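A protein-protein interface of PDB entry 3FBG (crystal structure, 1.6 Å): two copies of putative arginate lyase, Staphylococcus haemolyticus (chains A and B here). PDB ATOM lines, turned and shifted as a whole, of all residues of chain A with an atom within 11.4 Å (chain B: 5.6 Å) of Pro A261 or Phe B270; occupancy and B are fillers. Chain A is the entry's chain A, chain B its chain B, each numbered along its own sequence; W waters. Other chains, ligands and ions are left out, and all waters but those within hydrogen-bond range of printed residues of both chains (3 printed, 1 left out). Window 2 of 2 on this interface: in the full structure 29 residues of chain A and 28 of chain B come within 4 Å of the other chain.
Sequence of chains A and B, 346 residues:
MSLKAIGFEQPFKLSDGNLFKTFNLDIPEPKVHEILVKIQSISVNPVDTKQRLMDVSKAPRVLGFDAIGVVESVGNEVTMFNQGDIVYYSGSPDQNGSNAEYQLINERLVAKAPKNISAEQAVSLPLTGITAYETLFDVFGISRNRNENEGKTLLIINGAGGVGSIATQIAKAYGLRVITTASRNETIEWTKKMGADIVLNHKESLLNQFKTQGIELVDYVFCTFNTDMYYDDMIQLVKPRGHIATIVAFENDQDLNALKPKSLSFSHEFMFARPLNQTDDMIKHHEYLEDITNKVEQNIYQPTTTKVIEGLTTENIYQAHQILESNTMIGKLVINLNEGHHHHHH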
ATOM      1  N   LEU A 217     -13.085  15.160  16.680  1.00  0.00           N
ATOM      2  CA  LEU A 217     -13.564  15.037  15.301  1.00  0.00           C
ATOM      3  C   LEU A 217     -13.969  13.597  14.997  1.00  0.00           C
ATOM      4  O   LEU A 217     -13.232  12.663  15.345  1.00  0.00           O
ATOM      5  CB  LEU A 217     -12.518  15.549  14.330  1.00  0.00           C
ATOM      6  CG  LEU A 217     -12.076  16.998  14.571  1.00  0.00           C
ATOM      7  CD1 LEU A 217     -10.911  17.318  13.633  1.00  0.00           C
ATOM      8  CD2 LEU A 217     -13.237  18.031  14.378  1.00  0.00           C
ATOM      9  N   TYR A 231     -22.649  20.803   3.848  1.00  0.00           N
ATOM     10  CA  TYR A 231     -21.388  20.373   3.220  1.00  0.00           C
ATOM     11  C   TYR A 231     -20.148  20.870   3.980  1.00  0.00           C
ATOM     12  O   TYR A 231     -19.260  20.099   4.334  1.00  0.00           O
ATOM     13  CB  TYR A 231     -21.350  20.911   1.785  1.00  0.00           C
ATOM     14  CG  TYR A 231     -20.148  20.485   0.966  1.00  0.00           C
ATOM     15  CD1 TYR A 231     -20.001  19.155   0.555  1.00  0.00           C
ATOM     16  CD2 TYR A 231     -19.159  21.393   0.583  1.00  0.00           C
ATOM     17  CE1 TYR A 231     -18.898  18.756  -0.210  1.00  0.00           C
ATOM     18  CE2 TYR A 231     -18.073  21.022  -0.184  1.00  0.00           C
ATOM     19  CZ  TYR A 231     -17.946  19.728  -0.622  1.00  0.00           C
ATOM     20  OH  TYR A 231     -16.869  19.330  -1.346  1.00  0.00           O
ATOM     21  N   ASP A 232     -20.022  22.180   4.192  1.00  0.00           N
ATOM     22  CA  ASP A 232     -18.845  22.722   4.865  1.00  0.00           C
ATOM     23  C   ASP A 232     -18.754  22.297   6.321  1.00  0.00           C
ATOM     24  O   ASP A 232     -17.632  22.085   6.832  1.00  0.00           O
ATOM     25  CB  ASP A 232     -18.815  24.264   4.746  1.00  0.00           C
ATOM     26  CG  ASP A 232     -18.436  24.737   3.343  1.00  0.00           C
ATOM     27  OD1 ASP A 232     -17.805  23.980   2.576  1.00  0.00           O
ATOM     28  OD2 ASP A 232     -18.807  25.882   3.000  1.00  0.00           O
ATOM     29  N   MET A 234     -19.814  19.326   7.472  1.00  0.00           N
ATOM     30  CA  MET A 234     -19.332  17.906   7.462  1.00  0.00           C
ATOM     31  C   MET A 234     -17.816  17.886   7.331  1.00  0.00           C
ATOM     32  O   MET A 234     -17.137  17.108   8.007  1.00  0.00           O
ATOM     33  CB  MET A 234     -20.000  17.049   6.383  1.00  0.00           C
ATOM     34  CG  MET A 234     -21.505  16.627   6.616  1.00  0.00           C
ATOM     35  SD  MET A 234     -22.035  15.310   5.491  1.00  0.00           S
ATOM     36  CE  MET A 234     -22.375  16.694   4.260  1.00  0.00           C
ATOM     37  N   ILE A 235     -17.242  18.804   6.525  1.00  0.00           N
ATOM     38  CA  ILE A 235     -15.805  18.868   6.371  1.00  0.00           C
ATOM     39  C   ILE A 235     -15.143  19.323   7.692  1.00  0.00           C
ATOM     40  O   ILE A 235     -14.057  18.839   8.056  1.00  0.00           O
ATOM     41  CB  ILE A 235     -15.465  19.767   5.164  1.00  0.00           C
ATOM     42  CG1 ILE A 235     -15.956  19.021   3.911  1.00  0.00           C
ATOM     43  CG2 ILE A 235     -13.955  20.091   5.145  1.00  0.00           C
ATOM     44  CD1 ILE A 235     -15.753  19.875   2.625  1.00  0.00           C
ATOM     45  N   GLN A 236     -15.796  20.247   8.406  1.00  0.00           N
ATOM     46  CA  GLN A 236     -15.206  20.786   9.618  1.00  0.00           C
ATOM     47  C   GLN A 236     -15.206  19.730  10.710  1.00  0.00           C
ATOM     48  O   GLN A 236     -14.317  19.732  11.564  1.00  0.00           O
ATOM     49  CB  GLN A 236     -16.039  21.921  10.167  1.00  0.00           C
ATOM     50  CG  GLN A 236     -15.814  23.221   9.482  1.00  0.00           C
ATOM     51  CD  GLN A 236     -16.507  24.319  10.271  1.00  0.00           C
ATOM     52  OE1 GLN A 236     -15.853  25.195  10.844  1.00  0.00           O
ATOM     53  NE2 GLN A 236     -17.813  24.246  10.352  1.00  0.00           N
ATOM     54  N   LEU A 237     -16.221  18.902  10.708  1.00  0.00           N
ATOM     55  CA  LEU A 237     -16.444  18.053  11.905  1.00  0.00           C
ATOM     56  C   LEU A 237     -15.793  16.714  11.777  1.00  0.00           C
ATOM     57  O   LEU A 237     -15.696  15.980  12.787  1.00  0.00           O
ATOM     58  CB  LEU A 237     -17.954  17.852  12.109  1.00  0.00           C
ATOM     59  CG  LEU A 237     -18.704  19.185  12.324  1.00  0.00           C
ATOM     60  CD1 LEU A 237     -20.192  18.963  12.244  1.00  0.00           C
ATOM     61  CD2 LEU A 237     -18.283  19.757  13.702  1.00  0.00           C
ATOM     62  N   VAL A 238     -15.394  16.330  10.579  1.00  0.00           N
ATOM     63  CA  VAL A 238     -14.773  14.977  10.371  1.00  0.00           C
ATOM     64  C   VAL A 238     -13.248  15.013  10.613  1.00  0.00           C
ATOM     65  O   VAL A 238     -12.544  16.011  10.359  1.00  0.00           O
ATOM     66  CB  VAL A 238     -15.108  14.453   8.951  1.00  0.00           C
ATOM     67  CG1 VAL A 238     -14.228  15.187   7.893  1.00  0.00           C
ATOM     68  CG2 VAL A 238     -15.043  12.872   8.807  1.00  0.00           C
ATOM     69  N   LYS A 239     -12.690  13.892  11.081  1.00  0.00           N
ATOM     70  CA  LYS A 239     -11.264  13.785  11.258  1.00  0.00           C
ATOM     71  C   LYS A 239     -10.445  13.800   9.933  1.00  0.00           C
ATOM     72  O   LYS A 239     -10.958  13.441   8.852  1.00  0.00           O
ATOM     73  CB  LYS A 239     -10.994  12.518  12.135  1.00  0.00           C
ATOM     74  CG  LYS A 239     -11.026  11.278  11.378  1.00  0.00           C
ATOM     75  CD  LYS A 239     -10.934  10.072  12.327  1.00  0.00           C
ATOM     76  CE  LYS A 239      -9.731  10.122  13.272  1.00  0.00           C
ATOM     77  NZ  LYS A 239     -10.032   9.172  14.405  1.00  0.00           N
ATOM     78  N   PRO A 240      -9.142  14.147  10.020  1.00  0.00           N
ATOM     79  CA  PRO A 240      -8.300  14.058   8.828  1.00  0.00           C
ATOM     80  C   PRO A 240      -8.393  12.653   8.214  1.00  0.00           C
ATOM     81  O   PRO A 240      -8.370  11.666   8.951  1.00  0.00           O
ATOM     82  CB  PRO A 240      -6.884  14.294   9.381  1.00  0.00           C
ATOM     83  CG  PRO A 240      -7.133  15.238  10.596  1.00  0.00           C
ATOM     84  CD  PRO A 240      -8.419  14.675  11.193  1.00  0.00           C
ATOM     85  N   ARG A 241      -8.515  12.591   6.903  1.00  0.00           N
ATOM     86  CA  ARG A 241      -8.608  11.340   6.144  1.00  0.00           C
ATOM     87  C   ARG A 241      -9.926  10.621   6.378  1.00  0.00           C
ATOM     88  O   ARG A 241     -10.104   9.513   5.897  1.00  0.00           O
ATOM     89  CB  ARG A 241      -7.354  10.441   6.393  1.00  0.00           C
ATOM     90  CG  ARG A 241      -6.025  11.148   6.132  1.00  0.00           C
ATOM     91  CD  ARG A 241      -4.840  10.205   5.852  1.00  0.00           C
ATOM     92  NE  ARG A 241      -5.217   9.469   4.664  1.00  0.00           N
ATOM     93  CZ  ARG A 241      -4.993   9.901   3.427  1.00  0.00           C
ATOM     94  NH1 ARG A 241      -4.270  11.007   3.200  1.00  0.00           N
ATOM     95  NH2 ARG A 241      -5.505   9.225   2.406  1.00  0.00           N
ATOM     96  N   GLY A 242     -10.882  11.318   7.002  1.00  0.00           N
ATOM     97  CA  GLY A 242     -12.214  10.846   7.240  1.00  0.00           C
ATOM     98  C   GLY A 242     -13.119  10.762   6.010  1.00  0.00           C
ATOM     99  O   GLY A 242     -12.663  11.063   4.880  1.00  0.00           O
ATOM    100  N   ILE A 244     -17.121  11.494   4.458  1.00  0.00           N
ATOM    101  CA  ILE A 244     -18.410  12.152   4.548  1.00  0.00           C
ATOM    102  C   ILE A 244     -19.316  11.677   3.431  1.00  0.00           C
ATOM    103  O   ILE A 244     -18.792  11.272   2.374  1.00  0.00           O
ATOM    104  CB  ILE A 244     -18.270  13.725   4.547  1.00  0.00           C
ATOM    105  CG1 ILE A 244     -17.827  14.288   3.198  1.00  0.00           C
ATOM    106  CG2 ILE A 244     -17.328  14.217   5.680  1.00  0.00           C
ATOM    107  CD1 ILE A 244     -17.782  15.922   3.084  1.00  0.00           C
ATOM    108  N   ASP A 255     -17.561  22.858  -4.231  1.00  0.00           N
ATOM    109  CA  ASP A 255     -16.118  22.937  -4.404  1.00  0.00           C
ATOM    110  C   ASP A 255     -15.491  21.656  -3.886  1.00  0.00           C
ATOM    111  O   ASP A 255     -15.407  21.463  -2.654  1.00  0.00           O
ATOM    112  CB  ASP A 255     -15.574  24.090  -3.569  1.00  0.00           C
ATOM    113  CG  ASP A 255     -14.049  24.233  -3.674  1.00  0.00           C
ATOM    114  OD1 ASP A 255     -13.418  23.561  -4.508  1.00  0.00           O
ATOM    115  OD2 ASP A 255     -13.509  25.056  -2.908  1.00  0.00           O
ATOM    116  N   LEU A 256     -15.067  20.787  -4.797  1.00  0.00           N
ATOM    117  CA  LEU A 256     -14.433  19.527  -4.340  1.00  0.00           C
ATOM    118  C   LEU A 256     -13.035  19.745  -3.769  1.00  0.00           C
ATOM    119  O   LEU A 256     -12.476  18.855  -3.087  1.00  0.00           O
ATOM    120  CB  LEU A 256     -14.399  18.490  -5.446  1.00  0.00           C
ATOM    121  CG  LEU A 256     -15.745  17.868  -5.800  1.00  0.00           C
ATOM    122  CD1 LEU A 256     -15.555  16.975  -6.996  1.00  0.00           C
ATOM    123  CD2 LEU A 256     -16.317  17.048  -4.615  1.00  0.00           C
ATOM    124  N   ASN A 257     -12.450  20.913  -3.990  1.00  0.00           N
ATOM    125  CA  ASN A 257     -11.190  21.235  -3.321  1.00  0.00           C
ATOM    126  C   ASN A 257     -11.321  21.425  -1.823  1.00  0.00           C
ATOM    127  O   ASN A 257     -10.317  21.484  -1.114  1.00  0.00           O
ATOM    128  CB  ASN A 257     -10.521  22.464  -3.964  1.00  0.00           C
ATOM    129  CG  ASN A 257     -10.202  22.258  -5.396  1.00  0.00           C
ATOM    130  OD1 ASN A 257      -9.928  21.156  -5.865  1.00  0.00           O
ATOM    131  ND2 ASN A 257     -10.298  23.351  -6.164  1.00  0.00           N
ATOM    132  N   ALA A 258     -12.552  21.570  -1.340  1.00  0.00           N
ATOM    133  CA  ALA A 258     -12.778  21.746   0.106  1.00  0.00           C
ATOM    134  C   ALA A 258     -12.393  20.427   0.814  1.00  0.00           C
ATOM    135  O   ALA A 258     -12.094  20.482   1.998  1.00  0.00           O
ATOM    136  CB  ALA A 258     -14.201  22.116   0.355  1.00  0.00           C
ATOM    137  N   LEU A 259     -12.343  19.334   0.052  1.00  0.00           N
ATOM    138  CA  LEU A 259     -11.980  17.966   0.627  1.00  0.00           C
ATOM    139  C   LEU A 259     -10.476  17.860   0.746  1.00  0.00           C
ATOM    140  O   LEU A 259      -9.958  16.958   1.366  1.00  0.00           O
ATOM    141  CB  LEU A 259     -12.475  16.832  -0.297  1.00  0.00           C
ATOM    142  CG  LEU A 259     -13.993  16.840  -0.558  1.00  0.00           C
ATOM    143  CD1 LEU A 259     -14.352  15.846  -1.668  1.00  0.00           C
ATOM    144  CD2 LEU A 259     -14.789  16.574   0.719  1.00  0.00           C
ATOM    145  N   LYS A 260      -9.709  18.776   0.148  1.00  0.00           N
ATOM    146  CA  LYS A 260      -8.272  18.565   0.041  1.00  0.00           C
ATOM    147  C   LYS A 260      -7.465  18.689   1.336  1.00  0.00           C
ATOM    148  O   LYS A 260      -6.610  17.846   1.595  1.00  0.00           O
ATOM    149  CB  LYS A 260      -7.641  19.490  -1.028  1.00  0.00           C
ATOM    150  CG  LYS A 260      -6.144  19.231  -1.233  1.00  0.00           C
ATOM    151  CD  LYS A 260      -5.668  20.146  -2.395  1.00  0.00           C
ATOM    152  CE  LYS A 260      -4.146  20.183  -2.513  1.00  0.00           C
ATOM    153  NZ  LYS A 260      -3.729  20.904  -3.764  1.00  0.00           N
ATOM    154  N   PRO A 261      -7.687  19.749   2.148  1.00  0.00           N
ATOM    155  CA  PRO A 261      -6.805  19.931   3.327  1.00  0.00           C
ATOM    156  C   PRO A 261      -6.744  18.716   4.274  1.00  0.00           C
ATOM    157  O   PRO A 261      -5.651  18.426   4.828  1.00  0.00           O
ATOM    158  CB  PRO A 261      -7.454  21.111   4.069  1.00  0.00           C
ATOM    159  CG  PRO A 261      -7.979  21.958   2.902  1.00  0.00           C
ATOM    160  CD  PRO A 261      -8.572  20.918   1.938  1.00  0.00           C
ATOM    161  N   LYS A 262      -7.888  18.065   4.464  1.00  0.00           N
ATOM    162  CA  LYS A 262      -7.933  16.872   5.335  1.00  0.00           C
ATOM    163  C   LYS A 262      -7.896  15.576   4.518  1.00  0.00           C
ATOM    164  O   LYS A 262      -8.151  14.495   5.067  1.00  0.00           O
ATOM    165  CB  LYS A 262      -9.180  16.886   6.218  1.00  0.00           C
ATOM    166  CG  LYS A 262      -9.132  17.954   7.298  1.00  0.00           C
ATOM    167  CD  LYS A 262     -10.398  17.763   8.151  1.00  0.00           C
ATOM    168  CE  LYS A 262     -10.701  18.900   9.003  1.00  0.00           C
ATOM    169  NZ  LYS A 262     -11.927  18.580   9.769  1.00  0.00           N
ATOM    170  N   SER A 263      -7.616  15.671   3.212  1.00  0.00           N
ATOM    171  CA  SER A 263      -7.503  14.459   2.341  1.00  0.00           C
ATOM    172  C   SER A 263      -8.764  13.600   2.484  1.00  0.00           C
ATOM    173  O   SER A 263      -8.722  12.381   2.822  1.00  0.00           O
ATOM    174  CB  SER A 263      -6.210  13.670   2.642  1.00  0.00           C
ATOM    175  OG  SER A 263      -5.958  12.699   1.655  1.00  0.00           O
ATOM    176  N   LEU A 264      -9.925  14.232   2.324  1.00  0.00           N
ATOM    177  CA  LEU A 264     -11.202  13.547   2.608  1.00  0.00           C
ATOM    178  C   LEU A 264     -11.827  12.726   1.473  1.00  0.00           C
ATOM    179  O   LEU A 264     -11.567  13.001   0.307  1.00  0.00           O
ATOM    180  CB  LEU A 264     -12.250  14.562   3.084  1.00  0.00           C
ATOM    181  CG  LEU A 264     -11.907  15.396   4.313  1.00  0.00           C
ATOM    182  CD1 LEU A 264     -13.010  16.352   4.647  1.00  0.00           C
ATOM    183  CD2 LEU A 264     -11.682  14.438   5.542  1.00  0.00           C
ATOM    184  N   SER A 265     -12.722  11.799   1.824  1.00  0.00           N
ATOM    185  CA  SER A 265     -13.551  11.073   0.871  1.00  0.00           C
ATOM    186  C   SER A 265     -14.974  11.602   1.016  1.00  0.00           C
ATOM    187  O   SER A 265     -15.417  11.916   2.126  1.00  0.00           O
ATOM    188  CB  SER A 265     -13.542   9.532   1.181  1.00  0.00           C
ATOM    189  OG  SER A 265     -12.200   9.069   1.101  1.00  0.00           O
ATOM    190  N   GLN B  51       2.865  26.098  -4.021  1.00  0.00           N
ATOM    191  CA  GLN B  51       3.216  26.700  -2.737  1.00  0.00           C
ATOM    192  C   GLN B  51       3.974  28.022  -2.888  1.00  0.00           C
ATOM    193  O   GLN B  51       4.049  28.791  -1.948  1.00  0.00           O
ATOM    194  CB  GLN B  51       4.038  25.725  -1.875  1.00  0.00           C
ATOM    195  CG  GLN B  51       3.259  24.532  -1.327  1.00  0.00           C
ATOM    196  CD  GLN B  51       2.490  24.895  -0.082  1.00  0.00           C
ATOM    197  OE1 GLN B  51       2.720  25.955   0.500  1.00  0.00           O
ATOM    198  NE2 GLN B  51       1.563  24.025   0.338  1.00  0.00           N
ATOM    199  N   PRO B  93       4.706  21.280   4.383  1.00  0.00           N
ATOM    200  CA  PRO B  93       4.816  22.661   3.875  1.00  0.00           C
ATOM    201  C   PRO B  93       4.726  23.753   4.940  1.00  0.00           C
ATOM    202  O   PRO B  93       4.874  24.935   4.621  1.00  0.00           O
ATOM    203  CB  PRO B  93       3.652  22.763   2.866  1.00  0.00           C
ATOM    204  CG  PRO B  93       2.683  21.690   3.336  1.00  0.00           C
ATOM    205  CD  PRO B  93       3.522  20.579   3.844  1.00  0.00           C
ATOM    206  N   GLU B 134      -0.587   6.182  -0.192  1.00  0.00           N
ATOM    207  CA  GLU B 134      -1.810   6.642   0.494  1.00  0.00           C
ATOM    208  C   GLU B 134      -2.983   6.414  -0.425  1.00  0.00           C
ATOM    209  O   GLU B 134      -4.072   6.036   0.015  1.00  0.00           O
ATOM    210  CB  GLU B 134      -1.724   8.119   0.859  1.00  0.00           C
ATOM    211  CG  GLU B 134      -0.847   8.364   2.077  1.00  0.00           C
ATOM    212  CD  GLU B 134      -1.043   9.738   2.692  1.00  0.00           C
ATOM    213  OE1 GLU B 134      -1.379  10.670   1.931  1.00  0.00           O
ATOM    214  OE2 GLU B 134      -0.805   9.889   3.920  1.00  0.00           O
ATOM    215  N   HIS B 268     -10.208  13.260  -2.464  1.00  0.00           N
ATOM    216  CA  HIS B 268      -9.180  14.255  -2.851  1.00  0.00           C
ATOM    217  C   HIS B 268      -7.941  13.899  -2.030  1.00  0.00           C
ATOM    218  O   HIS B 268      -7.894  14.249  -0.845  1.00  0.00           O
ATOM    219  CB  HIS B 268      -9.640  15.665  -2.480  1.00  0.00           C
ATOM    220  CG  HIS B 268      -8.965  16.721  -3.311  1.00  0.00           C
ATOM    221  ND1 HIS B 268      -9.638  17.785  -3.899  1.00  0.00           N
ATOM    222  CD2 HIS B 268      -7.675  16.818  -3.708  1.00  0.00           C
ATOM    223  CE1 HIS B 268      -8.768  18.509  -4.580  1.00  0.00           C
ATOM    224  NE2 HIS B 268      -7.582  17.923  -4.520  1.00  0.00           N
ATOM    225  N   GLU B 269      -6.963  13.230  -2.655  1.00  0.00           N
ATOM    226  CA  GLU B 269      -5.765  12.800  -1.921  1.00  0.00           C
ATOM    227  C   GLU B 269      -4.791  13.967  -1.685  1.00  0.00           C
ATOM    228  O   GLU B 269      -4.458  14.696  -2.611  1.00  0.00           O
ATOM    229  CB  GLU B 269      -5.056  11.659  -2.649  1.00  0.00           C
ATOM    230  CG  GLU B 269      -3.581  11.426  -2.275  1.00  0.00           C
ATOM    231  CD  GLU B 269      -3.310  11.002  -0.813  1.00  0.00           C
ATOM    232  OE1 GLU B 269      -4.222  10.527  -0.099  1.00  0.00           O
ATOM    233  OE2 GLU B 269      -2.138  11.115  -0.389  1.00  0.00           O
ATOM    234  N   PHE B 270      -4.368  14.096  -0.431  1.00  0.00           N
ATOM    235  CA  PHE B 270      -3.417  15.140  -0.030  1.00  0.00           C
ATOM    236  C   PHE B 270      -2.453  14.517   0.976  1.00  0.00           C
ATOM    237  O   PHE B 270      -2.834  14.233   2.116  1.00  0.00           O
ATOM    238  CB  PHE B 270      -4.167  16.337   0.566  1.00  0.00           C
ATOM    239  CG  PHE B 270      -3.263  17.514   0.907  1.00  0.00           C
ATOM    240  CD1 PHE B 270      -2.270  17.925   0.027  1.00  0.00           C
ATOM    241  CD2 PHE B 270      -3.438  18.199   2.105  1.00  0.00           C
ATOM    242  CE1 PHE B 270      -1.441  19.044   0.345  1.00  0.00           C
ATOM    243  CE2 PHE B 270      -2.586  19.287   2.441  1.00  0.00           C
ATOM    244  CZ  PHE B 270      -1.605  19.705   1.528  1.00  0.00           C
ATOM    245  N   MET B 271      -1.196  14.286   0.576  1.00  0.00           N
ATOM    246  CA  MET B 271      -0.346  13.428   1.446  1.00  0.00           C
ATOM    247  C   MET B 271       0.068  14.164   2.706  1.00  0.00           C
ATOM    248  O   MET B 271       0.543  13.538   3.657  1.00  0.00           O
ATOM    249  CB  MET B 271       0.922  12.841   0.735  1.00  0.00           C
ATOM    250  CG  MET B 271       2.001  13.836   0.288  1.00  0.00           C
ATOM    251  SD  MET B 271       3.786  13.236   0.333  1.00  0.00           S
ATOM    252  CE  MET B 271       4.035  13.109   2.082  1.00  0.00           C
ATOM    253  N   PHE B 272      -0.110  15.480   2.710  1.00  0.00           N
ATOM    254  CA  PHE B 272       0.320  16.279   3.884  1.00  0.00           C
ATOM    255  C   PHE B 272      -0.739  16.385   4.968  1.00  0.00           C
ATOM    256  O   PHE B 272      -0.491  16.973   6.055  1.00  0.00           O
ATOM    257  CB  PHE B 272       0.842  17.667   3.430  1.00  0.00           C
ATOM    258  CG  PHE B 272       2.024  17.587   2.528  1.00  0.00           C
ATOM    259  CD1 PHE B 272       3.219  17.077   2.976  1.00  0.00           C
ATOM    260  CD2 PHE B 272       1.924  17.995   1.215  1.00  0.00           C
ATOM    261  CE1 PHE B 272       4.296  16.988   2.126  1.00  0.00           C
ATOM    262  CE2 PHE B 272       2.994  17.899   0.354  1.00  0.00           C
ATOM    263  CZ  PHE B 272       4.181  17.402   0.812  1.00  0.00           C
ATOM    264  N   ALA B 273      -1.902  15.754   4.752  1.00  0.00           N
ATOM    265  CA  ALA B 273      -2.926  15.766   5.775  1.00  0.00           C
ATOM    266  C   ALA B 273      -2.457  15.128   7.086  1.00  0.00           C
ATOM    267  O   ALA B 273      -2.717  15.663   8.156  1.00  0.00           O
ATOM    268  CB  ALA B 273      -4.231  15.096   5.282  1.00  0.00           C
ATOM    269  N   ARG B 274      -1.683  14.040   7.030  1.00  0.00           N
ATOM    270  CA  ARG B 274      -1.178  13.461   8.264  1.00  0.00           C
ATOM    271  C   ARG B 274      -0.205  14.390   9.090  1.00  0.00           C
ATOM    272  O   ARG B 274      -0.465  14.646  10.269  1.00  0.00           O
ATOM    273  CB  ARG B 274      -0.595  12.045   8.030  1.00  0.00           C
ATOM    274  CG  ARG B 274      -1.674  10.958   7.913  1.00  0.00           C
ATOM    275  CD  ARG B 274      -1.066   9.627   7.500  1.00  0.00           C
ATOM    276  NE  ARG B 274      -1.982   8.518   7.701  1.00  0.00           N
ATOM    277  CZ  ARG B 274      -2.244   7.611   6.768  1.00  0.00           C
ATOM    278  NH1 ARG B 274      -1.707   7.718   5.546  1.00  0.00           N
ATOM    279  NH2 ARG B 274      -3.042   6.629   7.041  1.00  0.00           N
ATOM    280  N   LEU B 276       0.493  17.688   8.718  1.00  0.00           N
ATOM    281  CA  LEU B 276      -0.130  18.987   8.981  1.00  0.00           C
ATOM    282  C   LEU B 276      -1.085  18.869  10.175  1.00  0.00           C
ATOM    283  O   LEU B 276      -1.179  19.768  11.034  1.00  0.00           O
ATOM    284  CB  LEU B 276      -0.831  19.537   7.734  1.00  0.00           C
ATOM    285  CG  LEU B 276      -0.041  20.102   6.545  1.00  0.00           C
ATOM    286  CD1 LEU B 276      -0.973  20.445   5.396  1.00  0.00           C
ATOM    287  CD2 LEU B 276       0.806  21.327   6.900  1.00  0.00           C
ATOM    288  N   ASN B 277      -1.781  17.750  10.269  1.00  0.00           N
ATOM    289  CA  ASN B 277      -2.682  17.570  11.393  1.00  0.00           C
ATOM    290  C   ASN B 277      -2.097  16.777  12.555  1.00  0.00           C
ATOM    291  O   ASN B 277      -2.823  16.356  13.448  1.00  0.00           O
ATOM    292  CB  ASN B 277      -4.030  16.975  10.923  1.00  0.00           C
ATOM    293  CG  ASN B 277      -4.832  17.944  10.096  1.00  0.00           C
ATOM    294  OD1 ASN B 277      -5.586  18.758  10.645  1.00  0.00           O
ATOM    295  ND2 ASN B 277      -4.683  17.881   8.766  1.00  0.00           N
HETATM  296  O   HOH W   1      -4.471  18.699  -4.979  1.00  0.00           O
HETATM  297  O   HOH W   2      -8.120  11.131   0.126  1.00  0.00           O
HETATM  298  O   HOH W   3      -5.454  19.946   7.151  1.00  0.00           O
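Water W1 lies within hydrogen-bond range of NZ of Lys A260 (2.6 Å) and NE2 of His B268 (3.2 Å). Water W3 bridges the side-chain amide nitrogen (ND2) of Asn B277 (2.7 Å) and the backbone carbonyl oxygen (O) of Pro A261 (2.8 Å). Water W2 lies within hydrogen-bond range of O of Ser A263 (3.0 Å) and O of His B268 (3.3 Å).
No position is printed for both chains.
Pro A261 touches just these residues of chain B: Phe B270 and Ala B273. Phe B270 touches four residues of chain A. No residue of chain A comes within 4 Å of Met B271. No residue of chain A comes within 4 Å of Phe B272. Ala B273 touches three residues of chain A. Printed residues of chain B within 4 Å of Asn A257: His B268 (3.2 Å). Of the printed residues of chain B, Lys A262 touches Ala B273. Leu A237 touches none of the printed residues of chain B. Gln B51 touches none of the printed residues of chain A. The nearest printed residue of chain B that does not touch Leu A264 is Glu B269 (5.5 Å).
Of the 24 printed residues of chain A, 10 touch a printed residue of chain B. Hydrophobic or aromatic side chains of chain A within 4 Å of the printed part of chain B: Pro A240 and Leu A259. Among the printed residues, Asp or Glu carboxylates within 4 Å of a Lys or Arg side-chain nitrogen of the other chain: Arg A241 with Glu B134 and Arg A241 with Glu B269.
Pro A240 touches Asn B277 (CG to CB, 3.6 Å). Phe B270 touches Arg A241. Asn A257 touches His B268. Leu A259 touches His B268 (CB to CB, 3.8 Å). His B268 touches Lys A260 (NE2 to CD, 3.6 Å). Lys A260 touches Phe B270. Phe B270 touches Pro A261. O of Pro A261 touches CB of Ala B273 (3.6 Å). C of Lys A262 touches CB of Ala B273, at 3.8 Å. CB of Ala B273 touches CB of Ser A263, at 3.6 Å.
NZ of Lys A262 lies within hydrogen-bond range of O of Ile A235, at 2.7 Å. The backbone carbonyl oxygen (O) of Gln A236 is in hydrogen-bond range of the side-chain amino group (NZ) of Lys A262 (3.2 Å). The backbone NH of Arg A241 is in hydrogen-bond range of the backbone carbonyl oxygen of Lys A262. NH1 of Arg A241 is in hydrogen-bond range of OG of Ser A263, at 2.8 Å. The guanidinium group (NH1) of Arg B274 lies within salt-bridge range of the side-chain carboxylate (OE2) of Glu B134, at 2.9 Å. The side-chain carboxylate (OE2) of Glu B269 sits at hydrogen-bond distance from the backbone NH (N) of Met B271 (3.4 Å).
NH1 of Arg A241 lies within salt-bridge range of OE1 of Glu B134 (3.2 Å). The guanidinium group (NH2) of Arg A241 is in salt-bridge range of the side-chain carboxylate (OE1) of Glu B269, 3.1 Å away. The backbone carbonyl oxygen (O) of Leu A256 sits at hydrogen-bond distance from a ring nitrogen (ND1) of His B268, at 3.1 Å. The side-chain hydroxyl (OG) of Ser A263 lies within hydrogen-bond range of the side-chain carboxylate (OE1) of Glu B269, 3.3 Å away. OG of Ser A263 is in hydrogen-bond range of N of Phe B270 (3.0 Å). The backbone NH (N) of His B268 sits at hydrogen-bond distance from the backbone carbonyl oxygen (O) of Leu A264, 3.1 Å away.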
